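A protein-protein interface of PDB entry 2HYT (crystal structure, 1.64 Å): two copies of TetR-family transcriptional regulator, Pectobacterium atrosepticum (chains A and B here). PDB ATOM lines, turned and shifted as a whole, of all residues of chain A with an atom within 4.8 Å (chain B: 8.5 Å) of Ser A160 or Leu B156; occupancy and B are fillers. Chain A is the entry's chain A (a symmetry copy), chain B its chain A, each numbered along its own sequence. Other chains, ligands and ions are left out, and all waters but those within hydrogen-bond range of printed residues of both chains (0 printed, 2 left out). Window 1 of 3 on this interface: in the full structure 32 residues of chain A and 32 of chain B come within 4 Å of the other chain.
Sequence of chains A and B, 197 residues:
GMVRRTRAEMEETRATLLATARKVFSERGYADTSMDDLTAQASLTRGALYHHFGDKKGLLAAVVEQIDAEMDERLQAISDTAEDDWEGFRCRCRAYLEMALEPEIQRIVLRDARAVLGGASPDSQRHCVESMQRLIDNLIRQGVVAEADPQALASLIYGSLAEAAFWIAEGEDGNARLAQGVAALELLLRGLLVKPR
The backbone carbonyl oxygen (O) of Leu B188 lies close to the backbone carbonyl oxygen (O) of Leu A188 (3.4 Å).
The side-chain hydroxyl of Ser B155 lies within hydrogen-bond range of the backbone carbonyl oxygen of Ala B152, at 2.6 Å. The side-chain hydroxyl (OG) of Ser B160 lies within hydrogen-bond range of the backbone carbonyl oxygen (O) of Ile B157 (2.7 Å). O of Ile A157 is in hydrogen-bond range of OG of Ser A160.
Leu B185 touches Leu A156. CB of Leu A156 touches CD1 of Leu B188, 3.8 Å away. Gly A159 touches Ser B160 (C to N, 3.7 Å). Gly A159 touches Glu B163 (CA to CB, 3.5 Å). Leu B156 touches Ser A160. CA of Ala A164 touches OG of Ser B155, 3.7 Å away. Leu B156 touches Gly A181. Leu B156 touches Leu A185. CB of Leu B156 touches CD1 of Leu A188, at 3.8 Å. Leu A188 touches Leu B192.
Of the printed residues of chain B, Ala A184 touches Leu B153 and Leu B156. Printed residues of chain B within 4 Å of Leu A156: Ser B160, Ala B164, Leu B185 and Leu B188. Printed residues of chain A within 4 Å of Leu B153: Ala A184 (3.99 Å). Ile B157 touches none of the printed residues of chain A. Leu B189 touches none of the printed residues of chain A. The nearest residue of chain A that does not touch Leu B156 is Leu A161 (4.5 Å). The nearest printed residue of chain B that does not touch Leu A156 is Leu B161 (4.5 Å).
Hydrophobic or aromatic side chains of chain B that line the printed part of chain A: Leu B156, Tyr B158, Ala B164, Leu B188 and Leu B192. Of the 13 printed residues of chain A, 10 touch a printed residue of chain B. Hydrophobic or aromatic side chains of chain A within 4 Å of the printed part of chain B: Leu A156, Tyr A158, Ala A164, Ala A184 and Leu A188. Among the printed residues, 23 pairs touch across the chains. Among the printed residues, no Asp or Glu carboxylate lies within 4 Å of a Lys or Arg side-chain nitrogen of the other chain.
Leu A156 touches Leu B185, and with the chains exchanged Leu A185 touches Leu B156. Leu A156 touches Leu B188, and with the chains exchanged Leu A188 touches Leu B156. Tyr A158 touches Glu B163, and with the chains exchanged Glu A163 touches Tyr B158. Gly A159 touches Ser B160, and with the chains exchanged Ser A160 touches Gly B159. Positions printed for both chains: 156, 157, 158, 159, 160, 161, 162, 163, 164, 185 and 188. Of the 23 pairs that touch across the chains among the printed residues, 17 have their exchanged pair printed and touching as well.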
ATOM      1  N   LEU A 156      26.861  18.677 -17.498  1.00  0.00           N
ATOM      2  CA  LEU A 156      25.667  18.197 -18.151  1.00  0.00           C
ATOM      3  C   LEU A 156      24.865  17.274 -17.222  1.00  0.00           C
ATOM      4  O   LEU A 156      23.672  17.465 -17.025  1.00  0.00           O
ATOM      5  CB  LEU A 156      26.005  17.466 -19.445  1.00  0.00           C
ATOM      6  CG  LEU A 156      26.464  18.392 -20.572  1.00  0.00           C
ATOM      7  CD1 LEU A 156      27.313  17.556 -21.587  1.00  0.00           C
ATOM      8  CD2 LEU A 156      25.298  19.081 -21.224  1.00  0.00           C
ATOM      9  N   ILE A 157      25.560  16.288 -16.655  1.00  0.00           N
ATOM     10  CA  ILE A 157      24.889  15.319 -15.774  1.00  0.00           C
ATOM     11  C   ILE A 157      24.282  15.987 -14.528  1.00  0.00           C
ATOM     12  O   ILE A 157      23.109  15.811 -14.228  1.00  0.00           O
ATOM     13  CB  ILE A 157      25.857  14.165 -15.378  1.00  0.00           C
ATOM     14  CG1 ILE A 157      26.288  13.360 -16.611  1.00  0.00           C
ATOM     15  CG2 ILE A 157      25.231  13.286 -14.297  1.00  0.00           C
ATOM     16  CD1 ILE A 157      27.457  12.390 -16.289  1.00  0.00           C
ATOM     17  N   TYR A 158      25.103  16.745 -13.810  1.00  0.00           N
ATOM     18  CA  TYR A 158      24.645  17.487 -12.635  1.00  0.00           C
ATOM     19  C   TYR A 158      23.424  18.356 -13.010  1.00  0.00           C
ATOM     20  O   TYR A 158      22.391  18.366 -12.302  1.00  0.00           O
ATOM     21  CB  TYR A 158      25.778  18.319 -11.984  1.00  0.00           C
ATOM     22  CG  TYR A 158      25.175  19.341 -11.029  1.00  0.00           C
ATOM     23  CD1 TYR A 158      24.666  18.927  -9.798  1.00  0.00           C
ATOM     24  CD2 TYR A 158      25.045  20.645 -11.361  1.00  0.00           C
ATOM     25  CE1 TYR A 158      24.048  19.818  -8.945  1.00  0.00           C
ATOM     26  CE2 TYR A 158      24.424  21.549 -10.525  1.00  0.00           C
ATOM     27  CZ  TYR A 158      23.975  21.133  -9.288  1.00  0.00           C
ATOM     28  OH  TYR A 158      23.379  22.041  -8.450  1.00  0.00           O
ATOM     29  N   GLY A 159      23.481  19.085 -14.154  1.00  0.00           N
ATOM     30  CA  GLY A 159      22.369  19.931 -14.572  1.00  0.00           C
ATOM     31  C   GLY A 159      21.090  19.138 -14.769  1.00  0.00           C
ATOM     32  O   GLY A 159      20.004  19.551 -14.361  1.00  0.00           O
ATOM     33  N   SER A 160      21.211  17.969 -15.385  1.00  0.00           N
ATOM     34  CA  SER A 160      20.021  17.150 -15.635  1.00  0.00           C
ATOM     35  C   SER A 160      19.363  16.756 -14.317  1.00  0.00           C
ATOM     36  O   SER A 160      18.133  16.819 -14.164  1.00  0.00           O
ATOM     37  CB  SER A 160      20.387  15.921 -16.462  1.00  0.00           C
ATOM     38  OG  SER A 160      21.090  14.904 -15.749  1.00  0.00           O
ATOM     39  N   LEU A 161      20.202  16.355 -13.375  1.00  0.00           N
ATOM     40  CA  LEU A 161      19.722  15.828 -12.094  1.00  0.00           C
ATOM     41  C   LEU A 161      19.105  16.934 -11.276  1.00  0.00           C
ATOM     42  O   LEU A 161      18.067  16.748 -10.671  1.00  0.00           O
ATOM     43  CB  LEU A 161      20.864  15.191 -11.324  1.00  0.00           C
ATOM     44  CG  LEU A 161      21.477  13.941 -11.940  1.00  0.00           C
ATOM     45  CD1 LEU A 161      22.716  13.481 -11.102  1.00  0.00           C
ATOM     46  CD2 LEU A 161      20.463  12.822 -12.027  1.00  0.00           C
ATOM     47  N   ALA A 162      19.761  18.101 -11.238  1.00  0.00           N
ATOM     48  CA  ALA A 162      19.269  19.229 -10.487  1.00  0.00           C
ATOM     49  C   ALA A 162      17.908  19.660 -10.996  1.00  0.00           C
ATOM     50  O   ALA A 162      16.972  19.906 -10.213  1.00  0.00           O
ATOM     51  CB  ALA A 162      20.278  20.384 -10.599  1.00  0.00           C
ATOM     52  N   GLU A 163      17.738  19.695 -12.315  1.00  0.00           N
ATOM     53  CA  GLU A 163      16.457  20.126 -12.860  1.00  0.00           C
ATOM     54  C   GLU A 163      15.352  19.084 -12.641  1.00  0.00           C
ATOM     55  O   GLU A 163      14.201  19.426 -12.302  1.00  0.00           O
ATOM     56  CB  GLU A 163      16.587  20.410 -14.368  1.00  0.00           C
ATOM     57  CG  GLU A 163      15.492  21.262 -14.923  1.00  0.00           C
ATOM     58  CD  GLU A 163      15.499  22.691 -14.341  1.00  0.00           C
ATOM     59  OE1 GLU A 163      16.526  23.131 -13.733  1.00  0.00           O
ATOM     60  OE2 GLU A 163      14.441  23.342 -14.459  1.00  0.00           O
ATOM     61  N   ALA A 164      15.701  17.833 -12.870  1.00  0.00           N
ATOM     62  CA  ALA A 164      14.743  16.746 -12.663  1.00  0.00           C
ATOM     63  C   ALA A 164      14.293  16.699 -11.192  1.00  0.00           C
ATOM     64  O   ALA A 164      13.133  16.436 -10.914  1.00  0.00           O
ATOM     65  CB  ALA A 164      15.314  15.430 -13.142  1.00  0.00           C
ATOM     66  N   GLY A 181      11.195  10.083 -13.839  1.00  0.00           N
ATOM     67  CA  GLY A 181      12.526  10.688 -13.910  1.00  0.00           C
ATOM     68  C   GLY A 181      13.648   9.684 -13.991  1.00  0.00           C
ATOM     69  O   GLY A 181      14.578   9.806 -14.807  1.00  0.00           O
ATOM     70  N   ALA A 184      13.632   7.961 -17.413  1.00  0.00           N
ATOM     71  CA  ALA A 184      14.160   8.829 -18.483  1.00  0.00           C
ATOM     72  C   ALA A 184      15.689   8.975 -18.307  1.00  0.00           C
ATOM     73  O   ALA A 184      16.457   8.937 -19.262  1.00  0.00           O
ATOM     74  CB  ALA A 184      13.474  10.177 -18.435  1.00  0.00           C
ATOM     75  N   LEU A 185      16.110   9.165 -17.061  1.00  0.00           N
ATOM     76  CA  LEU A 185      17.537   9.299 -16.751  1.00  0.00           C
ATOM     77  C   LEU A 185      18.345   8.120 -17.314  1.00  0.00           C
ATOM     78  O   LEU A 185      19.446   8.289 -17.872  1.00  0.00           O
ATOM     79  CB  LEU A 185      17.717   9.401 -15.248  1.00  0.00           C
ATOM     80  CG  LEU A 185      19.152   9.410 -14.727  1.00  0.00           C
ATOM     81  CD1 LEU A 185      19.905  10.676 -15.169  1.00  0.00           C
ATOM     82  CD2 LEU A 185      19.112   9.299 -13.188  1.00  0.00           C
ATOM     83  N   LEU A 188      19.229   8.575 -20.875  1.00  0.00           N
ATOM     84  CA  LEU A 188      20.353   9.499 -21.064  1.00  0.00           C
ATOM     85  C   LEU A 188      21.691   8.894 -20.679  1.00  0.00           C
ATOM     86  O   LEU A 188      22.719   9.120 -21.331  1.00  0.00           O
ATOM     87  CB  LEU A 188      20.178  10.752 -20.242  1.00  0.00           C
ATOM     88  CG  LEU A 188      19.309  11.865 -20.791  1.00  0.00           C
ATOM     89  CD1 LEU A 188      19.410  13.002 -19.813  1.00  0.00           C
ATOM     90  CD2 LEU A 188      19.731  12.291 -22.211  1.00  0.00           C
ATOM     91  N   VAL B 129      10.912  23.838 -20.584  1.00  0.00           N
ATOM     92  CA  VAL B 129      10.649  22.396 -20.522  1.00  0.00           C
ATOM     93  C   VAL B 129       9.437  22.028 -21.382  1.00  0.00           C
ATOM     94  O   VAL B 129       9.468  21.012 -22.068  1.00  0.00           O
ATOM     95  CB  VAL B 129      10.505  21.928 -19.078  1.00  0.00           C
ATOM     96  CG1 VAL B 129       9.929  20.530 -18.984  1.00  0.00           C
ATOM     97  CG2 VAL B 129      11.885  22.053 -18.361  1.00  0.00           C
ATOM     98  N   MET B 132      10.533  21.919 -25.059  1.00  0.00           N
ATOM     99  CA  MET B 132      11.292  20.706 -25.348  1.00  0.00           C
ATOM    100  C   MET B 132      10.412  19.459 -25.267  1.00  0.00           C
ATOM    101  O   MET B 132      10.583  18.515 -26.040  1.00  0.00           O
ATOM    102  CB  MET B 132      12.488  20.600 -24.399  1.00  0.00           C
ATOM    103  CG  MET B 132      13.261  19.332 -24.545  1.00  0.00           C
ATOM    104  SD  MET B 132      14.059  19.171 -26.294  1.00  0.00           S
ATOM    105  CE  MET B 132      15.399  20.637 -26.307  1.00  0.00           C
ATOM    106  N   ALA B 148       9.559   7.087 -22.973  1.00  0.00           N
ATOM    107  CA  ALA B 148       9.834   7.771 -21.727  1.00  0.00           C
ATOM    108  C   ALA B 148       8.756   8.810 -21.550  1.00  0.00           C
ATOM    109  O   ALA B 148       8.003   9.092 -22.492  1.00  0.00           O
ATOM    110  CB  ALA B 148      11.177   8.416 -21.770  1.00  0.00           C
ATOM    111  N   ASP B 149       8.601   9.337 -20.337  1.00  0.00           N
ATOM    112  CA  ASP B 149       7.671  10.423 -20.141  1.00  0.00           C
ATOM    113  C   ASP B 149       8.276  11.671 -20.775  1.00  0.00           C
ATOM    114  O   ASP B 149       9.375  12.087 -20.405  1.00  0.00           O
ATOM    115  CB  ASP B 149       7.390  10.697 -18.665  1.00  0.00           C
ATOM    116  CG  ASP B 149       6.422  11.825 -18.484  1.00  0.00           C
ATOM    117  OD1 ASP B 149       5.220  11.660 -18.875  1.00  0.00           O
ATOM    118  OD2 ASP B 149       6.834  12.883 -18.009  1.00  0.00           O
ATOM    119  N   PRO B 150       7.574  12.282 -21.733  1.00  0.00           N
ATOM    120  CA  PRO B 150       8.115  13.459 -22.364  1.00  0.00           C
ATOM    121  C   PRO B 150       8.527  14.580 -21.435  1.00  0.00           C
ATOM    122  O   PRO B 150       9.576  15.172 -21.642  1.00  0.00           O
ATOM    123  CB  PRO B 150       6.992  13.891 -23.342  1.00  0.00           C
ATOM    124  CG  PRO B 150       6.239  12.731 -23.590  1.00  0.00           C
ATOM    125  CD  PRO B 150       6.288  11.908 -22.336  1.00  0.00           C
ATOM    126  N   GLN B 151       7.708  14.882 -20.421  1.00  0.00           N
ATOM    127  CA  GLN B 151       8.001  16.000 -19.532  1.00  0.00           C
ATOM    128  C   GLN B 151       9.243  15.714 -18.669  1.00  0.00           C
ATOM    129  O   GLN B 151      10.082  16.592 -18.451  1.00  0.00           O
ATOM    130  CB  GLN B 151       6.841  16.373 -18.649  1.00  0.00           C
ATOM    131  CG  GLN B 151       6.999  17.784 -18.074  1.00  0.00           C
ATOM    132  CD  GLN B 151       5.731  18.278 -17.445  1.00  0.00           C
ATOM    133  OE1 GLN B 151       5.487  18.027 -16.281  1.00  0.00           O
ATOM    134  NE2 GLN B 151       4.883  18.954 -18.234  1.00  0.00           N
ATOM    135  N   ALA B 152       9.303  14.498 -18.153  1.00  0.00           N
ATOM    136  CA  ALA B 152      10.486  14.057 -17.392  1.00  0.00           C
ATOM    137  C   ALA B 152      11.777  14.158 -18.207  1.00  0.00           C
ATOM    138  O   ALA B 152      12.752  14.715 -17.765  1.00  0.00           O
ATOM    139  CB  ALA B 152      10.295  12.622 -16.908  1.00  0.00           C
ATOM    140  N   LEU B 153      11.735  13.663 -19.435  1.00  0.00           N
ATOM    141  CA  LEU B 153      12.910  13.664 -20.285  1.00  0.00           C
ATOM    142  C   LEU B 153      13.276  15.068 -20.684  1.00  0.00           C
ATOM    143  O   LEU B 153      14.434  15.423 -20.667  1.00  0.00           O
ATOM    144  CB  LEU B 153      12.691  12.775 -21.485  1.00  0.00           C
ATOM    145  CG  LEU B 153      13.845  12.634 -22.420  1.00  0.00           C
ATOM    146  CD1 LEU B 153      15.162  12.251 -21.668  1.00  0.00           C
ATOM    147  CD2 LEU B 153      13.525  11.581 -23.487  1.00  0.00           C
ATOM    148  N   ALA B 154      12.279  15.910 -20.947  1.00  0.00           N
ATOM    149  CA  ALA B 154      12.547  17.310 -21.273  1.00  0.00           C
ATOM    150  C   ALA B 154      13.198  18.034 -20.113  1.00  0.00           C
ATOM    151  O   ALA B 154      14.078  18.842 -20.324  1.00  0.00           O
ATOM    152  CB  ALA B 154      11.282  18.034 -21.748  1.00  0.00           C
ATOM    153  N   SER B 155      12.797  17.731 -18.869  1.00  0.00           N
ATOM    154  CA  SER B 155      13.403  18.364 -17.681  1.00  0.00           C
ATOM    155  C   SER B 155      14.880  18.044 -17.578  1.00  0.00           C
ATOM    156  O   SER B 155      15.694  18.915 -17.265  1.00  0.00           O
ATOM    157  CB  SER B 155      12.684  17.956 -16.388  1.00  0.00           C
ATOM    158  OG  SER B 155      12.959  16.621 -15.951  1.00  0.00           O
ATOM    159  N   LEU B 156      15.192  16.768 -17.794  1.00  0.00           N
ATOM    160  CA  LEU B 156      16.558  16.301 -17.766  1.00  0.00           C
ATOM    161  C   LEU B 156      17.399  16.999 -18.843  1.00  0.00           C
ATOM    162  O   LEU B 156      18.462  17.538 -18.558  1.00  0.00           O
ATOM    163  CB  LEU B 156      16.623  14.790 -17.953  1.00  0.00           C
ATOM    164  CG  LEU B 156      16.139  13.998 -16.738  1.00  0.00           C
ATOM    165  CD1 LEU B 156      15.699  12.574 -17.215  1.00  0.00           C
ATOM    166  CD2 LEU B 156      17.190  13.947 -15.664  1.00  0.00           C
ATOM    167  N   ILE B 157      16.885  16.982 -20.073  1.00  0.00           N
ATOM    168  CA  ILE B 157      17.621  17.589 -21.194  1.00  0.00           C
ATOM    169  C   ILE B 157      17.836  19.100 -21.000  1.00  0.00           C
ATOM    170  O   ILE B 157      18.951  19.594 -21.090  1.00  0.00           O
ATOM    171  CB  ILE B 157      16.915  17.291 -22.548  1.00  0.00           C
ATOM    172  CG1 ILE B 157      16.901  15.784 -22.842  1.00  0.00           C
ATOM    173  CG2 ILE B 157      17.554  18.098 -23.677  1.00  0.00           C
ATOM    174  CD1 ILE B 157      15.969  15.436 -24.035  1.00  0.00           C
ATOM    175  N   TYR B 158      16.749  19.818 -20.743  1.00  0.00           N
ATOM    176  CA  TYR B 158      16.814  21.257 -20.478  1.00  0.00           C
ATOM    177  C   TYR B 158      17.829  21.533 -19.346  1.00  0.00           C
ATOM    178  O   TYR B 158      18.699  22.427 -19.456  1.00  0.00           O
ATOM    179  CB  TYR B 158      15.422  21.865 -20.178  1.00  0.00           C
ATOM    180  CG  TYR B 158      15.592  23.241 -19.548  1.00  0.00           C
ATOM    181  CD1 TYR B 158      15.980  24.324 -20.337  1.00  0.00           C
ATOM    182  CD2 TYR B 158      15.451  23.446 -18.219  1.00  0.00           C
ATOM    183  CE1 TYR B 158      16.213  25.564 -19.783  1.00  0.00           C
ATOM    184  CE2 TYR B 158      15.686  24.677 -17.645  1.00  0.00           C
ATOM    185  CZ  TYR B 158      16.017  25.749 -18.449  1.00  0.00           C
ATOM    186  OH  TYR B 158      16.228  26.978 -17.875  1.00  0.00           O
ATOM    187  N   GLY B 159      17.781  20.754 -18.236  1.00  0.00           N
ATOM    188  CA  GLY B 159      18.704  20.957 -17.124  1.00  0.00           C
ATOM    189  C   GLY B 159      20.152  20.806 -17.550  1.00  0.00           C
ATOM    190  O   GLY B 159      21.023  21.589 -17.169  1.00  0.00           O
ATOM    191  N   SER B 160      20.424  19.800 -18.372  1.00  0.00           N
ATOM    192  CA  SER B 160      21.802  19.571 -18.814  1.00  0.00           C
ATOM    193  C   SER B 160      22.315  20.775 -19.597  1.00  0.00           C
ATOM    194  O   SER B 160      23.449  21.238 -19.402  1.00  0.00           O
ATOM    195  CB  SER B 160      21.888  18.293 -19.643  1.00  0.00           C
ATOM    196  OG  SER B 160      21.350  18.394 -20.961  1.00  0.00           O
ATOM    197  N   LEU B 161      21.458  21.272 -20.476  1.00  0.00           N
ATOM    198  CA  LEU B 161      21.839  22.350 -21.392  1.00  0.00           C
ATOM    199  C   LEU B 161      22.024  23.638 -20.629  1.00  0.00           C
ATOM    200  O   LEU B 161      22.963  24.369 -20.873  1.00  0.00           O
ATOM    201  CB  LEU B 161      20.778  22.532 -22.463  1.00  0.00           C
ATOM    202  CG  LEU B 161      20.599  21.375 -23.436  1.00  0.00           C
ATOM    203  CD1 LEU B 161      19.392  21.659 -24.391  1.00  0.00           C
ATOM    204  CD2 LEU B 161      21.857  21.142 -24.242  1.00  0.00           C
ATOM    205  N   ALA B 162      21.105  23.933 -19.701  1.00  0.00           N
ATOM    206  CA  ALA B 162      21.176  25.138 -18.911  1.00  0.00           C
ATOM    207  C   ALA B 162      22.453  25.169 -18.096  1.00  0.00           C
ATOM    208  O   ALA B 162      23.161  26.193 -18.042  1.00  0.00           O
ATOM    209  CB  ALA B 162      19.947  25.207 -17.991  1.00  0.00           C
ATOM    210  N   GLU B 163      22.822  24.038 -17.502  1.00  0.00           N
ATOM    211  CA  GLU B 163      24.028  24.018 -16.685  1.00  0.00           C
ATOM    212  C   GLU B 163      25.304  24.109 -17.532  1.00  0.00           C
ATOM    213  O   GLU B 163      26.266  24.820 -17.176  1.00  0.00           O
ATOM    214  CB  GLU B 163      24.079  22.733 -15.839  1.00  0.00           C
ATOM    215  CG  GLU B 163      25.006  22.810 -14.671  1.00  0.00           C
ATOM    216  CD  GLU B 163      24.555  23.849 -13.622  1.00  0.00           C
ATOM    217  OE1 GLU B 163      23.367  24.302 -13.640  1.00  0.00           O
ATOM    218  OE2 GLU B 163      25.425  24.238 -12.817  1.00  0.00           O
ATOM    219  N   ALA B 164      25.315  23.365 -18.622  1.00  0.00           N
ATOM    220  CA  ALA B 164      26.464  23.394 -19.528  1.00  0.00           C
ATOM    221  C   ALA B 164      26.668  24.809 -20.094  1.00  0.00           C
ATOM    222  O   ALA B 164      27.796  25.248 -20.256  1.00  0.00           O
ATOM    223  CB  ALA B 164      26.319  22.345 -20.610  1.00  0.00           C
ATOM    224  N   LEU B 185      27.731  16.360 -24.783  1.00  0.00           N
ATOM    225  CA  LEU B 185      26.284  16.337 -25.019  1.00  0.00           C
ATOM    226  C   LEU B 185      25.893  15.206 -25.982  1.00  0.00           C
ATOM    227  O   LEU B 185      24.889  14.495 -25.782  1.00  0.00           O
ATOM    228  CB  LEU B 185      25.843  17.681 -25.568  1.00  0.00           C
ATOM    229  CG  LEU B 185      24.385  17.801 -26.003  1.00  0.00           C
ATOM    230  CD1 LEU B 185      23.426  17.677 -24.807  1.00  0.00           C
ATOM    231  CD2 LEU B 185      24.202  19.156 -26.721  1.00  0.00           C
ATOM    232  N   LEU B 188      25.513  11.950 -24.271  1.00  0.00           N
ATOM    233  CA  LEU B 188      24.243  11.840 -23.545  1.00  0.00           C
ATOM    234  C   LEU B 188      23.050  11.638 -24.462  1.00  0.00           C
ATOM    235  O   LEU B 188      22.117  10.881 -24.162  1.00  0.00           O
ATOM    236  CB  LEU B 188      23.968  13.075 -22.724  1.00  0.00           C
ATOM    237  CG  LEU B 188      24.616  13.197 -21.359  1.00  0.00           C
ATOM    238  CD1 LEU B 188      24.082  14.463 -20.749  1.00  0.00           C
ATOM    239  CD2 LEU B 188      24.337  11.970 -20.468  1.00  0.00           C
ATOM    240  N   LEU B 189      23.042  12.323 -25.588  1.00  0.00           N
ATOM    241  CA  LEU B 189      21.856  12.271 -26.447  1.00  0.00           C
ATOM    242  C   LEU B 189      21.750  10.953 -27.184  1.00  0.00           C
ATOM    243  O   LEU B 189      20.660  10.490 -27.506  1.00  0.00           O
ATOM    244  CB  LEU B 189      21.870  13.421 -27.455  1.00  0.00           C
ATOM    245  CG  LEU B 189      21.813  14.830 -26.859  1.00  0.00           C
ATOM    246  CD1 LEU B 189      21.712  15.846 -27.983  1.00  0.00           C
ATOM    247  CD2 LEU B 189      20.639  15.009 -25.861  1.00  0.00           C
ATOM    248  N   LEU B 192      19.253   8.195 -26.217  1.00  0.00           N
ATOM    249  CA  LEU B 192      17.813   8.364 -26.426  1.00  0.00           C
ATOM    250  C   LEU B 192      17.276   7.604 -27.614  1.00  0.00           C
ATOM    251  O   LEU B 192      16.064   7.338 -27.665  1.00  0.00           O
ATOM    252  CB  LEU B 192      17.491   9.826 -26.602  1.00  0.00           C
ATOM    253  CG  LEU B 192      17.948  10.694 -25.426  1.00  0.00           C
ATOM    254  CD1 LEU B 192      17.390  12.091 -25.658  1.00  0.00           C
ATOM    255  CD2 LEU B 192      17.543  10.131 -24.100  1.00  0.00           C
